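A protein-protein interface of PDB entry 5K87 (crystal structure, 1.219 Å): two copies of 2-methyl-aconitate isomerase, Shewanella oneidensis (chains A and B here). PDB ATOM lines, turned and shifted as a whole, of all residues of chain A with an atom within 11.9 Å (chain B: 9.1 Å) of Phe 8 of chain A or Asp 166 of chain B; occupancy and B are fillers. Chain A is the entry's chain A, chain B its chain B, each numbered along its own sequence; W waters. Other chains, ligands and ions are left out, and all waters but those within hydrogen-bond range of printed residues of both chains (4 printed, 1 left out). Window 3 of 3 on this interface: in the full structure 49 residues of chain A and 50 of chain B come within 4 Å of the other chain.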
ATOM      1  N   LEU A   7      32.853  30.715  33.123  1.00  0.00           N
ATOM      2  CA  LEU A   7      32.713  29.506  33.930  1.00  0.00           C
ATOM      3  C   LEU A   7      31.747  28.508  33.288  1.00  0.00           C
ATOM      4  O   LEU A   7      31.580  27.391  33.776  1.00  0.00           O
ATOM      5  CB  LEU A   7      32.304  29.844  35.374  1.00  0.00           C
ATOM      6  CG  LEU A   7      30.903  30.326  35.790  1.00  0.00           C
ATOM      7  CD1 LEU A   7      30.268  31.289  34.783  1.00  0.00           C
ATOM      8  CD2 LEU A   7      29.969  29.153  36.120  1.00  0.00           C
ATOM      9  N   PHE A   8      31.132  28.928  32.187  1.00  0.00           N
ATOM     10  CA  PHE A   8      30.220  28.095  31.398  1.00  0.00           C
ATOM     11  C   PHE A   8      29.095  27.471  32.210  1.00  0.00           C
ATOM     12  O   PHE A   8      29.112  26.277  32.508  1.00  0.00           O
ATOM     13  CB  PHE A   8      30.996  27.072  30.574  1.00  0.00           C
ATOM     14  CG  PHE A   8      32.089  27.693  29.768  1.00  0.00           C
ATOM     15  CD1 PHE A   8      31.788  28.526  28.701  1.00  0.00           C
ATOM     16  CD2 PHE A   8      33.415  27.493  30.104  1.00  0.00           C
ATOM     17  CE1 PHE A   8      32.798  29.128  27.966  1.00  0.00           C
ATOM     18  CE2 PHE A   8      34.430  28.088  29.374  1.00  0.00           C
ATOM     19  CZ  PHE A   8      34.117  28.907  28.304  1.00  0.00           C
ATOM     20  N   PRO A   9      28.108  28.299  32.570  1.00  0.00           N
ATOM     21  CA  PRO A   9      26.938  27.837  33.314  1.00  0.00           C
ATOM     22  C   PRO A   9      26.141  26.832  32.491  1.00  0.00           C
ATOM     23  O   PRO A   9      26.269  26.796  31.262  1.00  0.00           O
ATOM     24  CB  PRO A   9      26.103  29.116  33.478  1.00  0.00           C
ATOM     25  CG  PRO A   9      27.025  30.245  33.196  1.00  0.00           C
ATOM     26  CD  PRO A   9      28.022  29.727  32.224  1.00  0.00           C
ATOM     27  N   PRO A  10      25.313  26.022  33.149  1.00  0.00           N
ATOM     28  CA  PRO A  10      24.443  25.131  32.380  1.00  0.00           C
ATOM     29  C   PRO A  10      23.483  25.899  31.481  1.00  0.00           C
ATOM     30  O   PRO A  10      23.201  27.074  31.708  1.00  0.00           O
ATOM     31  CB  PRO A  10      23.642  24.394  33.458  1.00  0.00           C
ATOM     32  CG  PRO A  10      24.405  24.588  34.731  1.00  0.00           C
ATOM     33  CD  PRO A  10      25.108  25.897  34.604  1.00  0.00           C
ATOM     34  N   GLN A  11      22.981  25.220  30.459  1.00  0.00           N
ATOM     35  CA  GLN A  11      21.958  25.810  29.612  1.00  0.00           C
ATOM     36  C   GLN A  11      20.709  26.064  30.437  1.00  0.00           C
ATOM     37  O   GLN A  11      20.407  25.330  31.385  1.00  0.00           O
ATOM     38  CB  GLN A  11      21.598  24.868  28.472  1.00  0.00           C
ATOM     39  CG  GLN A  11      22.711  24.591  27.484  1.00  0.00           C
ATOM     40  CD  GLN A  11      22.155  24.075  26.181  1.00  0.00           C
ATOM     41  OE1 GLN A  11      21.901  24.865  25.267  1.00  0.00           O
ATOM     42  NE2 GLN A  11      21.908  22.771  26.094  1.00  0.00           N
ATOM     43  N   ILE A  12      19.970  27.096  30.066  1.00  0.00           N
ATOM     44  CA  ILE A  12      18.642  27.313  30.630  1.00  0.00           C
ATOM     45  C   ILE A  12      17.611  26.495  29.856  1.00  0.00           C
ATOM     46  O   ILE A  12      17.844  26.104  28.707  1.00  0.00           O
ATOM     47  CB  ILE A  12      18.253  28.806  30.648  1.00  0.00           C
ATOM     48  CG1 ILE A  12      18.141  29.366  29.230  1.00  0.00           C
ATOM     49  CG2 ILE A  12      19.259  29.601  31.462  1.00  0.00           C
ATOM     50  CD1 ILE A  12      17.240  30.580  29.118  1.00  0.00           C
ATOM     51  N   ARG A  51      18.844  32.110  19.417  1.00  0.00           N
ATOM     52  CA  ARG A  51      19.615  30.977  19.889  1.00  0.00           C
ATOM     53  C   ARG A  51      18.796  29.691  19.876  1.00  0.00           C
ATOM     54  O   ARG A  51      19.326  28.626  19.586  1.00  0.00           O
ATOM     55  CB  ARG A  51      20.157  31.265  21.287  1.00  0.00           C
ATOM     56  CG  ARG A  51      21.267  30.337  21.709  1.00  0.00           C
ATOM     57  CD  ARG A  51      22.474  30.449  20.786  1.00  0.00           C
ATOM     58  NE  ARG A  51      23.424  29.387  21.081  1.00  0.00           N
ATOM     59  CZ  ARG A  51      23.318  28.152  20.609  1.00  0.00           C
ATOM     60  NH1 ARG A  51      22.310  27.831  19.798  1.00  0.00           N
ATOM     61  NH2 ARG A  51      24.227  27.247  20.928  1.00  0.00           N
ATOM     62  N   ASP A  64      22.684  23.850  14.877  1.00  0.00           N
ATOM     63  CA  ASP A  64      22.837  24.116  16.303  1.00  0.00           C
ATOM     64  C   ASP A  64      21.605  24.811  16.880  1.00  0.00           C
ATOM     65  O   ASP A  64      21.711  25.631  17.782  1.00  0.00           O
ATOM     66  CB  ASP A  64      24.100  24.937  16.547  1.00  0.00           C
ATOM     67  CG  ASP A  64      24.704  24.714  17.913  1.00  0.00           C
ATOM     68  OD1 ASP A  64      24.235  23.849  18.687  1.00  0.00           O
ATOM     69  OD2 ASP A  64      25.719  25.414  18.168  1.00  0.00           O
ATOM     70  N   ARG A 395      16.460  24.328  25.109  1.00  0.00           N
ATOM     71  CA  ARG A 395      17.606  24.793  25.873  1.00  0.00           C
ATOM     72  C   ARG A 395      18.461  25.749  25.076  1.00  0.00           C
ATOM     73  O   ARG A 395      18.646  25.567  23.869  1.00  0.00           O
ATOM     74  CB  ARG A 395      18.494  23.629  26.299  1.00  0.00           C
ATOM     75  CG  ARG A 395      17.832  22.616  27.179  1.00  0.00           C
ATOM     76  CD  ARG A 395      18.893  21.779  27.859  1.00  0.00           C
ATOM     77  NE  ARG A 395      18.315  20.602  28.495  1.00  0.00           N
ATOM     78  CZ  ARG A 395      19.027  19.628  29.049  1.00  0.00           C
ATOM     79  NH1 ARG A 395      20.345  19.696  29.076  1.00  0.00           N
ATOM     80  NH2 ARG A 395      18.413  18.583  29.586  1.00  0.00           N
ATOM     81  N   VAL A 396      19.005  26.748  25.761  1.00  0.00           N
ATOM     82  CA  VAL A 396      20.038  27.616  25.193  1.00  0.00           C
ATOM     83  C   VAL A 396      21.045  27.934  26.279  1.00  0.00           C
ATOM     84  O   VAL A 396      20.718  27.867  27.458  1.00  0.00           O
ATOM     85  CB  VAL A 396      19.478  28.956  24.632  1.00  0.00           C
ATOM     86  CG1 VAL A 396      18.536  28.705  23.464  1.00  0.00           C
ATOM     87  CG2 VAL A 396      18.796  29.772  25.719  1.00  0.00           C
ATOM     88  N   PRO A 397      22.278  28.282  25.893  1.00  0.00           N
ATOM     89  CA  PRO A 397      23.218  28.752  26.914  1.00  0.00           C
ATOM     90  C   PRO A 397      22.662  29.976  27.646  1.00  0.00           C
ATOM     91  O   PRO A 397      21.854  30.736  27.097  1.00  0.00           O
ATOM     92  CB  PRO A 397      24.474  29.091  26.098  1.00  0.00           C
ATOM     93  CG  PRO A 397      24.379  28.184  24.898  1.00  0.00           C
ATOM     94  CD  PRO A 397      22.907  28.165  24.568  1.00  0.00           C
ATOM     95  N   LYS A 398      23.085  30.147  28.893  1.00  0.00           N
ATOM     96  CA  LYS A 398      22.540  31.189  29.748  1.00  0.00           C
ATOM     97  C   LYS A 398      22.827  32.544  29.125  1.00  0.00           C
ATOM     98  O   LYS A 398      23.964  32.814  28.746  1.00  0.00           O
ATOM     99  CB  LYS A 398      23.156  31.088  31.143  1.00  0.00           C
ATOM    100  CG  LYS A 398      22.566  32.049  32.161  1.00  0.00           C
ATOM    101  CD  LYS A 398      23.309  31.962  33.488  1.00  0.00           C
ATOM    102  CE  LYS A 398      22.792  32.996  34.478  1.00  0.00           C
ATOM    103  NZ  LYS A 398      23.638  33.077  35.699  1.00  0.00           N
ATOM    104  N   PRO A 399      21.784  33.382  28.980  1.00  0.00           N
ATOM    105  CA  PRO A 399      21.893  34.727  28.399  1.00  0.00           C
ATOM    106  C   PRO A 399      22.881  35.615  29.150  1.00  0.00           C
ATOM    107  O   PRO A 399      23.057  35.487  30.362  1.00  0.00           O
ATOM    108  CB  PRO A 399      20.476  35.286  28.554  1.00  0.00           C
ATOM    109  CG  PRO A 399      19.599  34.078  28.565  1.00  0.00           C
ATOM    110  CD  PRO A 399      20.387  33.035  29.298  1.00  0.00           C
ATOM    111  OXT PRO A 399      23.521  36.489  28.562  1.00  0.00           O
ATOM    112  N   THR B 157      30.314  18.518  35.452  1.00  0.00           N
ATOM    113  CA  THR B 157      30.390  19.567  36.460  1.00  0.00           C
ATOM    114  C   THR B 157      29.234  19.367  37.431  1.00  0.00           C
ATOM    115  O   THR B 157      28.089  19.236  37.002  1.00  0.00           O
ATOM    116  CB  THR B 157      30.272  20.958  35.819  1.00  0.00           C
ATOM    117  OG1 THR B 157      31.360  21.144  34.913  1.00  0.00           O
ATOM    118  CG2 THR B 157      30.301  22.050  36.865  1.00  0.00           C
ATOM    119  N   ASP B 158      29.546  19.306  38.727  1.00  0.00           N
ATOM    120  CA  ASP B 158      28.540  19.118  39.779  1.00  0.00           C
ATOM    121  C   ASP B 158      27.624  17.931  39.491  1.00  0.00           C
ATOM    122  O   ASP B 158      26.411  18.006  39.698  1.00  0.00           O
ATOM    123  CB  ASP B 158      27.723  20.395  39.996  1.00  0.00           C
ATOM    124  CG  ASP B 158      28.579  21.565  40.429  1.00  0.00           C
ATOM    125  OD1 ASP B 158      29.328  21.423  41.415  1.00  0.00           O
ATOM    126  OD2 ASP B 158      28.514  22.625  39.777  1.00  0.00           O
ATOM    127  N   VAL B 161      26.288  16.501  33.113  1.00  0.00           N
ATOM    128  CA  VAL B 161      27.034  16.769  31.890  1.00  0.00           C
ATOM    129  C   VAL B 161      27.298  18.269  31.745  1.00  0.00           C
ATOM    130  O   VAL B 161      26.386  19.097  31.884  1.00  0.00           O
ATOM    131  CB  VAL B 161      26.291  16.253  30.651  1.00  0.00           C
ATOM    132  CG1 VAL B 161      26.967  16.727  29.360  1.00  0.00           C
ATOM    133  CG2 VAL B 161      26.198  14.730  30.677  1.00  0.00           C
ATOM    134  N   GLN B 162      28.553  18.615  31.480  1.00  0.00           N
ATOM    135  CA  GLN B 162      28.937  19.969  31.113  1.00  0.00           C
ATOM    136  C   GLN B 162      28.758  20.111  29.603  1.00  0.00           C
ATOM    137  O   GLN B 162      29.537  19.570  28.822  1.00  0.00           O
ATOM    138  CB  GLN B 162      30.394  20.230  31.527  1.00  0.00           C
ATOM    139  CG  GLN B 162      30.946  21.604  31.126  1.00  0.00           C
ATOM    140  CD  GLN B 162      30.273  22.744  31.863  1.00  0.00           C
ATOM    141  OE1 GLN B 162      30.144  22.711  33.088  1.00  0.00           O
ATOM    142  NE2 GLN B 162      29.834  23.761  31.128  1.00  0.00           N
ATOM    143  N   GLU B 163      27.701  20.812  29.200  1.00  0.00           N
ATOM    144  CA  GLU B 163      27.367  20.962  27.783  1.00  0.00           C
ATOM    145  C   GLU B 163      28.062  22.164  27.164  1.00  0.00           C
ATOM    146  O   GLU B 163      28.564  22.099  26.040  1.00  0.00           O
ATOM    147  CB  GLU B 163      25.865  21.161  27.610  1.00  0.00           C
ATOM    148  CG  GLU B 163      24.988  20.035  28.114  1.00  0.00           C
ATOM    149  CD  GLU B 163      23.554  20.236  27.660  1.00  0.00           C
ATOM    150  OE1 GLU B 163      22.848  21.096  28.233  1.00  0.00           O
ATOM    151  OE2 GLU B 163      23.147  19.545  26.709  1.00  0.00           O
ATOM    152  N   THR B 164      28.070  23.269  27.898  1.00  0.00           N
ATOM    153  CA  THR B 164      28.533  24.543  27.374  1.00  0.00           C
ATOM    154  C   THR B 164      30.051  24.671  27.528  1.00  0.00           C
ATOM    155  O   THR B 164      30.662  24.009  28.368  1.00  0.00           O
ATOM    156  CB  THR B 164      27.838  25.696  28.094  1.00  0.00           C
ATOM    157  OG1 THR B 164      28.079  25.582  29.506  1.00  0.00           O
ATOM    158  CG2 THR B 164      26.318  25.662  27.831  1.00  0.00           C
ATOM    159  N   GLY B 165      30.667  25.521  26.715  1.00  0.00           N
ATOM    160  CA  GLY B 165      32.113  25.626  26.714  1.00  0.00           C
ATOM    161  C   GLY B 165      32.601  26.468  25.561  1.00  0.00           C
ATOM    162  O   GLY B 165      31.798  27.078  24.856  1.00  0.00           O
ATOM    163  N   ASP B 166      33.917  26.496  25.354  1.00  0.00           N
ATOM    164  CA  ASP B 166      34.492  27.348  24.317  1.00  0.00           C
ATOM    165  C   ASP B 166      35.162  26.587  23.183  1.00  0.00           C
ATOM    166  O   ASP B 166      35.937  27.168  22.415  1.00  0.00           O
ATOM    167  CB  ASP B 166      35.467  28.377  24.919  1.00  0.00           C
ATOM    168  CG  ASP B 166      36.641  27.737  25.640  1.00  0.00           C
ATOM    169  OD1 ASP B 166      36.827  26.507  25.558  1.00  0.00           O
ATOM    170  OD2 ASP B 166      37.396  28.487  26.296  1.00  0.00           O
ATOM    171  N   PHE B 167      34.869  25.300  23.060  1.00  0.00           N
ATOM    172  CA  PHE B 167      35.463  24.502  21.999  1.00  0.00           C
ATOM    173  C   PHE B 167      34.677  24.651  20.705  1.00  0.00           C
ATOM    174  O   PHE B 167      33.459  24.431  20.669  1.00  0.00           O
ATOM    175  CB  PHE B 167      35.533  23.030  22.404  1.00  0.00           C
ATOM    176  CG  PHE B 167      36.356  22.181  21.474  1.00  0.00           C
ATOM    177  CD1 PHE B 167      37.738  22.277  21.475  1.00  0.00           C
ATOM    178  CD2 PHE B 167      35.759  21.274  20.612  1.00  0.00           C
ATOM    179  CE1 PHE B 167      38.509  21.499  20.624  1.00  0.00           C
ATOM    180  CE2 PHE B 167      36.532  20.489  19.760  1.00  0.00           C
ATOM    181  CZ  PHE B 167      37.904  20.605  19.773  1.00  0.00           C
ATOM    182  N   GLU B 168      35.382  25.009  19.637  1.00  0.00           N
ATOM    183  CA  GLU B 168      34.771  25.239  18.336  1.00  0.00           C
ATOM    184  C   GLU B 168      34.993  24.058  17.399  1.00  0.00           C
ATOM    185  O   GLU B 168      36.076  23.463  17.374  1.00  0.00           O
ATOM    186  CB  GLU B 168      35.366  26.495  17.693  1.00  0.00           C
ATOM    187  CG  GLU B 168      35.346  27.730  18.572  1.00  0.00           C
ATOM    188  CD  GLU B 168      34.151  28.618  18.299  1.00  0.00           C
ATOM    189  OE1 GLU B 168      33.273  28.202  17.513  1.00  0.00           O
ATOM    190  OE2 GLU B 168      34.096  29.733  18.864  1.00  0.00           O
ATOM    191  N   LEU B 169      33.954  23.723  16.642  1.00  0.00           N
ATOM    192  CA  LEU B 169      34.018  22.719  15.585  1.00  0.00           C
ATOM    193  C   LEU B 169      33.661  23.418  14.287  1.00  0.00           C
ATOM    194  O   LEU B 169      32.673  24.146  14.240  1.00  0.00           O
ATOM    195  CB  LEU B 169      32.960  21.629  15.809  1.00  0.00           C
ATOM    196  CG  LEU B 169      33.236  20.340  16.579  1.00  0.00           C
ATOM    197  CD1 LEU B 169      33.671  20.650  17.976  1.00  0.00           C
ATOM    198  CD2 LEU B 169      32.000  19.452  16.597  1.00  0.00           C
ATOM    199  N   PHE B 174      28.005  27.433  17.128  1.00  0.00           N
ATOM    200  CA  PHE B 174      28.370  28.004  18.415  1.00  0.00           C
ATOM    201  C   PHE B 174      29.304  27.072  19.184  1.00  0.00           C
ATOM    202  O   PHE B 174      29.213  25.855  19.078  1.00  0.00           O
ATOM    203  CB  PHE B 174      27.086  28.256  19.205  1.00  0.00           C
ATOM    204  CG  PHE B 174      26.141  29.205  18.515  1.00  0.00           C
ATOM    205  CD1 PHE B 174      26.430  30.552  18.462  1.00  0.00           C
ATOM    206  CD2 PHE B 174      24.978  28.756  17.908  1.00  0.00           C
ATOM    207  CE1 PHE B 174      25.579  31.441  17.821  1.00  0.00           C
ATOM    208  CE2 PHE B 174      24.122  29.649  17.258  1.00  0.00           C
ATOM    209  CZ  PHE B 174      24.429  30.985  17.221  1.00  0.00           C
ATOM    210  N   PRO B 175      30.219  27.645  19.968  1.00  0.00           N
ATOM    211  CA  PRO B 175      31.105  26.786  20.762  1.00  0.00           C
ATOM    212  C   PRO B 175      30.352  26.027  21.863  1.00  0.00           C
ATOM    213  O   PRO B 175      29.287  26.436  22.313  1.00  0.00           O
ATOM    214  CB  PRO B 175      32.113  27.775  21.366  1.00  0.00           C
ATOM    215  CG  PRO B 175      31.438  29.097  21.324  1.00  0.00           C
ATOM    216  CD  PRO B 175      30.497  29.079  20.152  1.00  0.00           C
ATOM    217  N   ALA B 176      30.940  24.924  22.299  1.00  0.00           N
ATOM    218  CA  ALA B 176      30.382  24.107  23.372  1.00  0.00           C
ATOM    219  C   ALA B 176      31.533  23.364  24.059  1.00  0.00           C
ATOM    220  O   ALA B 176      32.687  23.567  23.720  1.00  0.00           O
ATOM    221  CB  ALA B 176      29.330  23.133  22.814  1.00  0.00           C
ATOM    222  N   ALA B 177      31.238  22.511  25.030  1.00  0.00           N
ATOM    223  CA  ALA B 177      32.296  21.769  25.697  1.00  0.00           C
ATOM    224  C   ALA B 177      32.895  20.728  24.761  1.00  0.00           C
ATOM    225  O   ALA B 177      32.175  20.026  24.055  1.00  0.00           O
ATOM    226  CB  ALA B 177      31.750  21.091  26.933  1.00  0.00           C
ATOM    227  N   GLU B 178      34.216  20.596  24.780  1.00  0.00           N
ATOM    228  CA  GLU B 178      34.891  19.555  24.021  1.00  0.00           C
ATOM    229  C   GLU B 178      34.538  18.169  24.550  1.00  0.00           C
ATOM    230  O   GLU B 178      34.547  17.942  25.764  1.00  0.00           O
ATOM    231  CB  GLU B 178      36.404  19.756  24.106  1.00  0.00           C
ATOM    232  CG  GLU B 178      37.201  18.826  23.210  1.00  0.00           C
ATOM    233  CD  GLU B 178      38.705  19.054  23.271  1.00  0.00           C
ATOM    234  OE1 GLU B 178      39.165  19.953  24.013  1.00  0.00           O
ATOM    235  OE2 GLU B 178      39.425  18.316  22.572  1.00  0.00           O
ATOM    236  N   ARG B 384      34.743  16.229  19.355  1.00  0.00           N
ATOM    237  CA  ARG B 384      33.480  16.781  18.898  1.00  0.00           C
ATOM    238  C   ARG B 384      32.888  17.582  20.061  1.00  0.00           C
ATOM    239  O   ARG B 384      33.618  18.018  20.952  1.00  0.00           O
ATOM    240  CB  ARG B 384      32.544  15.666  18.418  1.00  0.00           C
ATOM    241  CG  ARG B 384      33.093  14.786  17.269  1.00  0.00           C
ATOM    242  CD  ARG B 384      32.819  15.348  15.870  1.00  0.00           C
ATOM    243  NE  ARG B 384      33.732  16.419  15.480  1.00  0.00           N
ATOM    244  CZ  ARG B 384      33.627  17.105  14.344  1.00  0.00           C
ATOM    245  NH1 ARG B 384      34.512  18.048  14.053  1.00  0.00           N
ATOM    246  NH2 ARG B 384      32.635  16.846  13.500  1.00  0.00           N
ATOM    247  N   SER B 385      31.577  17.816  20.015  1.00  0.00           N
ATOM    248  CA  SER B 385      30.842  18.482  21.090  1.00  0.00           C
ATOM    249  C   SER B 385      29.385  18.098  20.909  1.00  0.00           C
ATOM    250  O   SER B 385      29.018  17.556  19.865  1.00  0.00           O
ATOM    251  CB  SER B 385      30.997  20.001  21.025  1.00  0.00           C
ATOM    252  OG  SER B 385      30.297  20.553  19.914  1.00  0.00           O
HETATM  253  O   HOH W   1      26.994  24.555  20.350  1.00  0.00           O
HETATM  254  O   HOH W   2      23.574  22.398  30.442  1.00  0.00           O
HETATM  255  O   HOH W   3      26.106  26.351  22.377  1.00  0.00           O
HETATM  256  O   HOH W   4      28.595  24.946  35.140  1.00  0.00           O
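No position is printed for both chains. Of the 10 pairs that touch across the chains among the printed residues, none has its exchanged pair printed and touching as well.
Printed residues of chain B within 4 Å of Phe 8 of chain A: Gln 162 (3.0 Å), Thr 164 (3.2 Å), Gly 165 (3.5 Å) and Asp 166 (3.7 Å). Asp 166 of chain B touches just one residue of chain A: Phe 8. Of chain A, only Phe 8 (3.2 Å), Pro 9 (2.8 Å) and Gln 11 (3.8 Å) come within 4 Å of Thr 164 of chain B. Of chain A, only Phe 8 (3.5 Å) comes within 4 Å of Gly 165 of chain B. Phe 167 of chain B touches none of the printed residues of chain A. No residue of chain A comes within 4 Å of Glu 168 of chain B. No residue of chain A comes within 4 Å of Pro 175 of chain B. Ala 176 of chain B touches none of the printed residues of chain A. Of the printed residues of chain B, Gln 11 of chain A touches Glu 163 and Thr 164. Of the printed residues of chain B, Asp 64 of chain A touches Phe 174. Of the printed residues of chain A, Glu 163 of chain B touches Gln 11 (2.9 Å) and Arg 395 (3.0 Å). The nearest residue of chain A that does not touch Asp 166 of chain B is Leu 7 of chain A (8.5 Å).
O of Phe 8 of chain A sits at hydrogen-bond distance from NE2 of Gln 162 of chain B, at 3.0 Å. OG1 of Thr 164 of chain B is in hydrogen-bond range of O of Phe 8 of chain A. O of Pro 9 of chain A is in hydrogen-bond range of OG1 of Thr 164 of chain B, at 2.8 Å. The side-chain amide nitrogen (NE2) of Gln 11 of chain A sits at hydrogen-bond distance from the side-chain carboxylate (OE1) of Glu 163 of chain B (2.9 Å). OD2 of Asp 64 of chain A sits at hydrogen-bond distance from N of Phe 174 of chain B, at 3.2 Å. The guanidinium group (NH1) of Arg 395 of chain A is in salt-bridge range of the side-chain carboxylate (OE1) of Glu 163 of chain B.
Water W3 lies within hydrogen-bond range of NH2 of Arg 51 of chain A (2.5 Å) and O of Pro 175 of chain B (3.2 Å). Water W2 bridges the side-chain carboxylate of Glu 163 of chain B and the backbone NH of Gln 11 of chain A. Water W1 lies within hydrogen-bond range of the side-chain carboxylate of Asp 64 of chain A (2.7 Å) and the backbone carbonyl oxygen of Phe 174 of chain B (2.9 Å). Water W4 lies within hydrogen-bond range of the backbone carbonyl oxygen (O) of Phe 8 of chain A and the side-chain amide oxygen (OE1) of Gln 162 of chain B.
Among the printed residues, merely in contact across the chains: Arg 51 of chain A with Phe 174 of chain B (3.2 Å), Phe 8 of chain A with Gly 165 of chain B (3.5 Å), Phe 8 of chain A with Asp 166 of chain B (3.7 Å) and Gln 11 of chain A with Thr 164 of chain B (3.8 Å).
Of the 13 printed residues of chain A, 6 touch a printed residue of chain B. Of the 18 printed residues of chain B, 6 touch a printed residue of chain A. Printed residues of chain B that touch a printed residue of chain A: Gln 162, Glu 163, Thr 164, Gly 165, Asp 166 and Phe 174. Along chain B the printed residues that touch a printed residue of chain A span positions 162 to 174. Among the printed residues, Asp or Glu carboxylates within 4 Å of a Lys or Arg side-chain nitrogen of the other chain: Arg 395 of chain A with Glu 163 of chain B (3.0 Å).
The side-chain amide oxygen of Gln 11 of chain A sits close to the backbone NH of Val 396 of chain A, 3.5 Å away. The guanidinium group (NH2) of Arg 51 of chain A lies within salt-bridge range of the side-chain carboxylate (OD2) of Asp 64 of chain A (3.6 Å). The side-chain hydroxyl (OG1) of Thr 157 of chain B is in hydrogen-bond range of the side-chain amide oxygen (OE1) of Gln 162 of chain B (2.7 Å). NE2 of Gln 162 of chain B lies within hydrogen-bond range of O of Thr 164 of chain B (2.9 Å). The backbone carbonyl oxygen (O) of Glu 163 of chain B lies within hydrogen-bond range of the backbone NH (N) of Ala 177 of chain B (2.9 Å). The backbone carbonyl oxygen (O) of Gly 165 of chain B is in hydrogen-bond range of the backbone NH (N) of Ala 176 of chain B.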
